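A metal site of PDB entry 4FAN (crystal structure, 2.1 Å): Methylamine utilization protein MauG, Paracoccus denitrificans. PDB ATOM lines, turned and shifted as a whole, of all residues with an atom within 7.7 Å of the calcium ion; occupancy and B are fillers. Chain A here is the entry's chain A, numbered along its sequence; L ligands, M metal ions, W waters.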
ATOM      1  N   ARG A  39     -17.531  33.592  -1.902  1.00  0.00           N
ATOM      2  CA  ARG A  39     -17.942  32.192  -1.711  1.00  0.00           C
ATOM      3  C   ARG A  39     -17.789  31.345  -2.983  1.00  0.00           C
ATOM      4  O   ARG A  39     -18.672  30.516  -3.333  1.00  0.00           O
ATOM      5  CB  ARG A  39     -19.364  32.056  -1.197  1.00  0.00           C
ATOM      6  CG  ARG A  39     -19.528  30.767  -0.343  1.00  0.00           C
ATOM      7  CD  ARG A  39     -20.936  30.591   0.188  1.00  0.00           C
ATOM      8  NE  ARG A  39     -21.146  29.449   1.095  1.00  0.00           N
ATOM      9  CZ  ARG A  39     -21.572  28.251   0.738  1.00  0.00           C
ATOM     10  NH1 ARG A  39     -21.763  27.966  -0.539  1.00  0.00           N
ATOM     11  NH2 ARG A  39     -21.766  27.309   1.660  1.00  0.00           N
ATOM     12  N   THR A  42     -20.944  31.306  -5.283  1.00  0.00           N
ATOM     13  CA  THR A  42     -22.187  30.619  -4.899  1.00  0.00           C
ATOM     14  C   THR A  42     -22.830  31.482  -3.829  1.00  0.00           C
ATOM     15  O   THR A  42     -22.273  32.522  -3.449  1.00  0.00           O
ATOM     16  CB  THR A  42     -21.962  29.202  -4.357  1.00  0.00           C
ATOM     17  OG1 THR A  42     -21.140  29.236  -3.173  1.00  0.00           O
ATOM     18  CG2 THR A  42     -21.344  28.287  -5.404  1.00  0.00           C
ATOM     19  N   ASP A  43     -23.978  31.012  -3.321  1.00  0.00           N
ATOM     20  CA  ASP A  43     -24.846  31.882  -2.569  1.00  0.00           C
ATOM     21  C   ASP A  43     -24.675  31.618  -1.086  1.00  0.00           C
ATOM     22  O   ASP A  43     -25.070  30.528  -0.612  1.00  0.00           O
ATOM     23  CB  ASP A  43     -26.301  31.722  -3.004  1.00  0.00           C
ATOM     24  CG  ASP A  43     -27.206  32.848  -2.430  1.00  0.00           C
ATOM     25  OD1 ASP A  43     -28.398  32.963  -2.817  1.00  0.00           O
ATOM     26  OD2 ASP A  43     -26.713  33.627  -1.561  1.00  0.00           O
ATOM     27  N   LEU A  51     -29.349  26.799   2.621  1.00  0.00           N
ATOM     28  CA  LEU A  51     -28.496  27.214   1.531  1.00  0.00           C
ATOM     29  C   LEU A  51     -28.731  26.345   0.302  1.00  0.00           C
ATOM     30  O   LEU A  51     -28.072  26.522  -0.713  1.00  0.00           O
ATOM     31  CB  LEU A  51     -27.024  27.144   1.965  1.00  0.00           C
ATOM     32  CG  LEU A  51     -26.319  28.358   2.601  1.00  0.00           C
ATOM     33  CD1 LEU A  51     -27.276  29.404   3.151  1.00  0.00           C
ATOM     34  CD2 LEU A  51     -25.389  27.887   3.729  1.00  0.00           C
ATOM     35  N   ALA A  52     -29.702  25.446   0.390  1.00  0.00           N
ATOM     36  CA  ALA A  52     -30.013  24.520  -0.696  1.00  0.00           C
ATOM     37  C   ALA A  52     -30.381  25.262  -1.989  1.00  0.00           C
ATOM     38  O   ALA A  52     -29.878  24.907  -3.068  1.00  0.00           O
ATOM     39  CB  ALA A  52     -31.104  23.496  -0.309  1.00  0.00           C
ATOM     40  N   ASN A  66     -29.662  24.195  -6.465  1.00  0.00           N
ATOM     41  CA  ASN A  66     -28.560  24.835  -5.743  1.00  0.00           C
ATOM     42  C   ASN A  66     -27.803  25.636  -6.783  1.00  0.00           C
ATOM     43  O   ASN A  66     -27.616  25.166  -7.956  1.00  0.00           O
ATOM     44  CB  ASN A  66     -27.675  23.772  -5.125  1.00  0.00           C
ATOM     45  CG  ASN A  66     -26.502  24.342  -4.355  1.00  0.00           C
ATOM     46  OD1 ASN A  66     -25.318  24.116  -4.721  1.00  0.00           O
ATOM     47  ND2 ASN A  66     -26.805  25.083  -3.275  1.00  0.00           N
ATOM     48  N   THR A  67     -27.426  26.840  -6.356  1.00  0.00           N
ATOM     49  CA  THR A  67     -26.636  27.740  -7.114  1.00  0.00           C
ATOM     50  C   THR A  67     -25.215  27.192  -7.267  1.00  0.00           C
ATOM     51  O   THR A  67     -24.494  27.082  -6.295  1.00  0.00           O
ATOM     52  CB  THR A  67     -26.623  29.104  -6.399  1.00  0.00           C
ATOM     53  OG1 THR A  67     -27.935  29.683  -6.436  1.00  0.00           O
ATOM     54  CG2 THR A  67     -25.557  30.078  -7.069  1.00  0.00           C
ATOM     55  N   PRO A  68     -24.800  26.841  -8.514  1.00  0.00           N
ATOM     56  CA  PRO A  68     -23.462  26.298  -8.622  1.00  0.00           C
ATOM     57  C   PRO A  68     -22.375  27.410  -8.702  1.00  0.00           C
ATOM     58  O   PRO A  68     -22.638  28.580  -9.094  1.00  0.00           O
ATOM     59  CB  PRO A  68     -23.516  25.489  -9.971  1.00  0.00           C
ATOM     60  CG  PRO A  68     -24.446  26.360 -10.841  1.00  0.00           C
ATOM     61  CD  PRO A  68     -25.493  26.924  -9.817  1.00  0.00           C
ATOM     62  N   THR A  69     -21.148  27.056  -8.339  1.00  0.00           N
ATOM     63  CA  THR A  69     -19.976  27.935  -8.563  1.00  0.00           C
ATOM     64  C   THR A  69     -19.849  28.328 -10.061  1.00  0.00           C
ATOM     65  O   THR A  69     -20.212  27.542 -10.941  1.00  0.00           O
ATOM     66  CB  THR A  69     -18.713  27.194  -8.240  1.00  0.00           C
ATOM     67  OG1 THR A  69     -17.626  28.079  -8.429  1.00  0.00           O
ATOM     68  CG2 THR A  69     -18.561  25.957  -9.282  1.00  0.00           C
ATOM     69  N   TRP A  93     -27.528  22.849 -14.420  1.00  0.00           N
ATOM     70  CA  TRP A  93     -27.448  21.464 -14.016  1.00  0.00           C
ATOM     71  C   TRP A  93     -28.092  20.536 -15.027  1.00  0.00           C
ATOM     72  O   TRP A  93     -27.786  19.344 -15.059  1.00  0.00           O
ATOM     73  CB  TRP A  93     -28.130  21.285 -12.703  1.00  0.00           C
ATOM     74  CG  TRP A  93     -27.436  21.827 -11.520  1.00  0.00           C
ATOM     75  CD1 TRP A  93     -27.751  22.994 -10.870  1.00  0.00           C
ATOM     76  CD2 TRP A  93     -26.409  21.202 -10.759  1.00  0.00           C
ATOM     77  NE1 TRP A  93     -26.956  23.131  -9.769  1.00  0.00           N
ATOM     78  CE2 TRP A  93     -26.134  22.047  -9.659  1.00  0.00           C
ATOM     79  CE3 TRP A  93     -25.692  19.984 -10.889  1.00  0.00           C
ATOM     80  CZ2 TRP A  93     -25.125  21.744  -8.700  1.00  0.00           C
ATOM     81  CZ3 TRP A  93     -24.689  19.680  -9.899  1.00  0.00           C
ATOM     82  CH2 TRP A  93     -24.437  20.555  -8.815  1.00  0.00           C
ATOM     83  N   VAL A 272     -15.018  22.266  -4.530  1.00  0.00           N
ATOM     84  CA  VAL A 272     -16.179  21.536  -4.019  1.00  0.00           C
ATOM     85  C   VAL A 272     -16.174  21.646  -2.485  1.00  0.00           C
ATOM     86  O   VAL A 272     -17.239  21.625  -1.874  1.00  0.00           O
ATOM     87  CB  VAL A 272     -16.255  20.109  -4.452  1.00  0.00           C
ATOM     88  CG1 VAL A 272     -15.087  19.245  -3.864  1.00  0.00           C
ATOM     89  CG2 VAL A 272     -17.614  19.492  -4.138  1.00  0.00           C
ATOM     90  N   VAL A 274     -15.860  24.105  -0.655  1.00  0.00           N
ATOM     91  CA  VAL A 274     -16.363  25.321  -0.083  1.00  0.00           C
ATOM     92  C   VAL A 274     -17.702  25.721  -0.690  1.00  0.00           C
ATOM     93  O   VAL A 274     -18.206  26.796  -0.346  1.00  0.00           O
ATOM     94  CB  VAL A 274     -15.309  26.522  -0.165  1.00  0.00           C
ATOM     95  CG1 VAL A 274     -13.941  26.105   0.366  1.00  0.00           C
ATOM     96  CG2 VAL A 274     -15.167  26.981  -1.561  1.00  0.00           C
ATOM     97  N   THR A 275     -18.295  24.890  -1.564  1.00  0.00           N
ATOM     98  CA  THR A 275     -19.560  25.284  -2.214  1.00  0.00           C
ATOM     99  C   THR A 275     -20.758  24.415  -1.772  1.00  0.00           C
ATOM    100  O   THR A 275     -21.761  24.218  -2.486  1.00  0.00           O
ATOM    101  CB  THR A 275     -19.429  25.206  -3.719  1.00  0.00           C
ATOM    102  OG1 THR A 275     -18.906  23.921  -4.053  1.00  0.00           O
ATOM    103  CG2 THR A 275     -18.504  26.281  -4.239  1.00  0.00           C
ATOM    104  N   GLY A 276     -20.668  23.851  -0.590  1.00  0.00           N
ATOM    105  CA  GLY A 276     -21.853  23.235   0.040  1.00  0.00           C
ATOM    106  C   GLY A 276     -23.031  24.207   0.026  1.00  0.00           C
ATOM    107  O   GLY A 276     -22.838  25.419  -0.106  1.00  0.00           O
ATOM    108  N   PRO A 277     -24.255  23.672   0.128  1.00  0.00           N
ATOM    109  CA  PRO A 277     -24.571  22.252   0.151  1.00  0.00           C
ATOM    110  C   PRO A 277     -24.377  21.601  -1.263  1.00  0.00           C
ATOM    111  O   PRO A 277     -23.872  22.271  -2.195  1.00  0.00           O
ATOM    112  CB  PRO A 277     -26.017  22.225   0.662  1.00  0.00           C
ATOM    113  CG  PRO A 277     -26.567  23.535   0.343  1.00  0.00           C
ATOM    114  CD  PRO A 277     -25.465  24.519   0.206  1.00  0.00           C
ATOM    115  N   TYR A 278     -24.683  20.297  -1.400  1.00  0.00           N
ATOM    116  CA  TYR A 278     -24.292  19.594  -2.615  1.00  0.00           C
ATOM    117  C   TYR A 278     -25.385  19.061  -3.508  1.00  0.00           C
ATOM    118  O   TYR A 278     -26.557  19.078  -3.172  1.00  0.00           O
ATOM    119  CB  TYR A 278     -23.209  18.549  -2.334  1.00  0.00           C
ATOM    120  CG  TYR A 278     -22.012  19.196  -1.708  1.00  0.00           C
ATOM    121  CD1 TYR A 278     -21.853  19.165  -0.315  1.00  0.00           C
ATOM    122  CD2 TYR A 278     -21.116  19.969  -2.468  1.00  0.00           C
ATOM    123  CE1 TYR A 278     -20.790  19.799   0.292  1.00  0.00           C
ATOM    124  CE2 TYR A 278     -20.055  20.593  -1.871  1.00  0.00           C
ATOM    125  CZ  TYR A 278     -19.903  20.492  -0.469  1.00  0.00           C
ATOM    126  OH  TYR A 278     -18.880  21.082   0.194  1.00  0.00           O
ATOM    127  N   MET A 279     -24.964  18.587  -4.680  1.00  0.00           N
ATOM    128  CA  MET A 279     -25.872  18.053  -5.684  1.00  0.00           C
ATOM    129  C   MET A 279     -26.776  19.123  -6.228  1.00  0.00           C
ATOM    130  O   MET A 279     -26.840  20.240  -5.661  1.00  0.00           O
ATOM    131  CB  MET A 279     -26.695  16.909  -5.112  1.00  0.00           C
ATOM    132  CG  MET A 279     -25.795  15.790  -4.600  1.00  0.00           C
ATOM    133  SD  MET A 279     -24.525  15.246  -5.741  1.00  0.00           S
ATOM    134  CE  MET A 279     -23.522  14.207  -4.646  1.00  0.00           C
ATOM    135  N   HIS A 280     -27.513  18.774  -7.264  1.00  0.00           N
ATOM    136  CA  HIS A 280     -28.302  19.764  -7.991  1.00  0.00           C
ATOM    137  C   HIS A 280     -29.343  20.444  -7.096  1.00  0.00           C
ATOM    138  O   HIS A 280     -29.837  21.516  -7.433  1.00  0.00           O
ATOM    139  CB  HIS A 280     -28.974  19.156  -9.240  1.00  0.00           C
ATOM    140  CG  HIS A 280     -30.022  18.155  -8.900  1.00  0.00           C
ATOM    141  ND1 HIS A 280     -29.789  16.800  -8.915  1.00  0.00           N
ATOM    142  CD2 HIS A 280     -31.296  18.326  -8.470  1.00  0.00           C
ATOM    143  CE1 HIS A 280     -30.893  16.166  -8.531  1.00  0.00           C
ATOM    144  NE2 HIS A 280     -31.806  17.063  -8.238  1.00  0.00           N
ATOM    145  N   ASN A 281     -29.677  19.831  -5.977  1.00  0.00           N
ATOM    146  CA  ASN A 281     -30.740  20.351  -5.124  1.00  0.00           C
ATOM    147  C   ASN A 281     -30.260  20.769  -3.728  1.00  0.00           C
ATOM    148  O   ASN A 281     -31.088  21.073  -2.840  1.00  0.00           O
ATOM    149  CB  ASN A 281     -31.897  19.347  -5.019  1.00  0.00           C
ATOM    150  CG  ASN A 281     -31.445  17.996  -4.502  1.00  0.00           C
ATOM    151  OD1 ASN A 281     -30.346  17.864  -4.009  1.00  0.00           O
ATOM    152  ND2 ASN A 281     -32.294  16.988  -4.620  1.00  0.00           N
ATOM    153  N   GLY A 282     -28.936  20.796  -3.561  1.00  0.00           N
ATOM    154  CA  GLY A 282     -28.356  21.211  -2.293  1.00  0.00           C
ATOM    155  C   GLY A 282     -28.809  20.286  -1.216  1.00  0.00           C
ATOM    156  O   GLY A 282     -28.795  20.672  -0.069  1.00  0.00           O
ATOM    157  N   PHE A 284     -27.640  17.732   0.347  1.00  0.00           N
ATOM    158  CA  PHE A 284     -26.630  17.357   1.364  1.00  0.00           C
ATOM    159  C   PHE A 284     -25.829  18.604   1.731  1.00  0.00           C
ATOM    160  O   PHE A 284     -25.298  19.293   0.836  1.00  0.00           O
ATOM    161  CB  PHE A 284     -25.656  16.280   0.851  1.00  0.00           C
ATOM    162  CG  PHE A 284     -26.316  15.108   0.188  1.00  0.00           C
ATOM    163  CD1 PHE A 284     -27.416  14.477   0.774  1.00  0.00           C
ATOM    164  CD2 PHE A 284     -25.805  14.607  -0.999  1.00  0.00           C
ATOM    165  CE1 PHE A 284     -28.021  13.415   0.157  1.00  0.00           C
ATOM    166  CE2 PHE A 284     -26.410  13.515  -1.617  1.00  0.00           C
ATOM    167  CZ  PHE A 284     -27.531  12.923  -1.026  1.00  0.00           C
HETATM  168 FE1  LIG L   1     -19.927  12.359  -8.306  1.00  0.00          FE
HETATM  169  C1  LIG L   1     -21.909  15.110  -7.740  1.00  0.00           C
HETATM  170  C2  LIG L   1     -17.950  13.189  -5.733  1.00  0.00           C
HETATM  171  C3  LIG L   1     -18.541   9.164  -8.383  1.00  0.00           C
HETATM  172  C4  LIG L   1     -21.203  11.936 -11.345  1.00  0.00           C
HETATM  173  N1  LIG L   1     -19.960  13.905  -6.908  1.00  0.00           N
HETATM  174  C5  LIG L   1     -20.764  14.934  -6.850  1.00  0.00           C
HETATM  175  C6  LIG L   1     -20.481  15.827  -5.699  1.00  0.00           C
HETATM  176  C7  LIG L   1     -19.349  15.291  -5.084  1.00  0.00           C
HETATM  177  C8  LIG L   1     -19.106  14.079  -5.937  1.00  0.00           C
HETATM  178  C9  LIG L   1     -18.520  15.726  -3.897  1.00  0.00           C
HETATM  179  C10 LIG L   1     -21.263  17.067  -5.405  1.00  0.00           C
HETATM  180  C11 LIG L   1     -20.473  18.166  -6.126  1.00  0.00           C
HETATM  181  C12 LIG L   1     -21.223  19.471  -6.179  1.00  0.00           C
HETATM  182  O1  LIG L   1     -22.393  19.456  -5.774  1.00  0.00           O
HETATM  183  O2  LIG L   1     -20.673  20.534  -6.638  1.00  0.00           O
HETATM  184  N2  LIG L   1     -18.495  11.353  -7.249  1.00  0.00           N
HETATM  185  C13 LIG L   1     -17.770  11.843  -6.257  1.00  0.00           C
HETATM  186  C14 LIG L   1     -16.812  10.903  -5.667  1.00  0.00           C
HETATM  187  C15 LIG L   1     -16.982   9.767  -6.429  1.00  0.00           C
HETATM  188  C16 LIG L   1     -18.049  10.107  -7.367  1.00  0.00           C
HETATM  189  C17 LIG L   1     -15.864  11.163  -4.537  1.00  0.00           C
HETATM  190  C18 LIG L   1     -16.331   8.427  -6.300  1.00  0.00           C
HETATM  191  C19 LIG L   1     -16.776   8.020  -4.892  1.00  0.00           C
HETATM  192  N3  LIG L   1     -19.853  10.834  -9.690  1.00  0.00           N
HETATM  193  C20 LIG L   1     -19.324   9.610  -9.547  1.00  0.00           C
HETATM  194  C21 LIG L   1     -19.582   8.737 -10.671  1.00  0.00           C
HETATM  195  C22 LIG L   1     -20.336   9.513 -11.533  1.00  0.00           C
HETATM  196  C23 LIG L   1     -20.475  10.793 -10.836  1.00  0.00           C
HETATM  197  C24 LIG L   1     -19.119   7.311 -10.777  1.00  0.00           C
HETATM  198  C25 LIG L   1     -20.938   9.179 -12.855  1.00  0.00           C
HETATM  199  C26 LIG L   1     -21.676   7.899 -12.595  1.00  0.00           C
HETATM  200  N4  LIG L   1     -21.332  13.387  -9.377  1.00  0.00           N
HETATM  201  C27 LIG L   1     -21.855  12.979 -10.542  1.00  0.00           C
HETATM  202  C28 LIG L   1     -23.032  13.727 -10.960  1.00  0.00           C
HETATM  203  C29 LIG L   1     -23.205  14.623  -9.926  1.00  0.00           C
HETATM  204  C30 LIG L   1     -22.129  14.372  -8.977  1.00  0.00           C
HETATM  205  C31 LIG L   1     -23.874  13.513 -12.177  1.00  0.00           C
HETATM  206  C32 LIG L   1     -24.307  15.600  -9.781  1.00  0.00           C
HETATM  207  C33 LIG L   1     -25.384  14.643  -9.302  1.00  0.00           C
HETATM  208  C34 LIG L   1     -26.567  15.549  -9.166  1.00  0.00           C
HETATM  209  O3  LIG L   1     -26.434  16.586  -8.462  1.00  0.00           O
HETATM  210  O4  LIG L   1     -27.590  15.217  -9.780  1.00  0.00           O
HETATM  211 CA    CA M   1     -23.379  23.636  -3.994  1.00  0.00          CA
HETATM  212  O   HOH W   1     -21.208  22.651  -4.549  1.00  0.00           O
HETATM  213  O   HOH W   2     -23.927  21.788  -5.469  1.00  0.00           O
HETATM  214  O   HOH W   3     -24.124  25.627  -2.655  1.00  0.00           O
HETATM  215  O   HOH W   4     -22.695  25.420  -5.413  1.00  0.00           O
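The calcium ion is bound by the side-chain amide oxygen (OD1) of Asn 66 (2.1 Å), the backbone carbonyl oxygen (O) of Thr 275 (2.3 Å), the backbone carbonyl oxygen (O) of Pro 277 (2.3 Å), water W4 (2.4 Å), water W2 (2.4 Å), water W1 (2.4 Å) and water W3 (2.5 Å). The calcium ion has seven donor atoms within binding distance.
O of Asn 66 is in hydrogen-bond range of NE1 of Trp 93 (2.8 Å). The side-chain amide nitrogen (ND2) of Asn 66 is in hydrogen-bond range of the backbone carbonyl oxygen (O) of Leu 51. O of Ala 52 lies close to ND2 of Asn 66 (3.1 Å). The backbone carbonyl oxygen (O) of His 280 lies within hydrogen-bond range of the backbone NH (N) of Asn 66, 2.9 Å away.
Water W1 bridges the side-chain hydroxyl of Thr 275 and an oxygen (O2) of the ligand. Water W3 lies within hydrogen-bond range of the side-chain amide nitrogen (ND2) of Asn 66 (2.8 Å) and the backbone carbonyl oxygen (O) of Gly 276 (2.9 Å). Water W2 bridges O1 of the ligand and O of Met 279.
O1 of the ligand sits at hydrogen-bond distance from N of Met 279, at 2.9 Å. The backbone NH (N) of His 280 sits at hydrogen-bond distance from an oxygen (O3) of the ligand, at 2.7 Å. A ring nitrogen (ND1) of His 280 is in hydrogen-bond range of an oxygen (O4) of the ligand (2.8 Å).
Of the 21 residues printed, 3 come within 4 Å of the calcium ion. Along chain A the residues within 4 Å of the calcium ion span positions 66 to 277. The nearest printed residue that does not touch the calcium ion is Gly 276 (4.1 Å).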
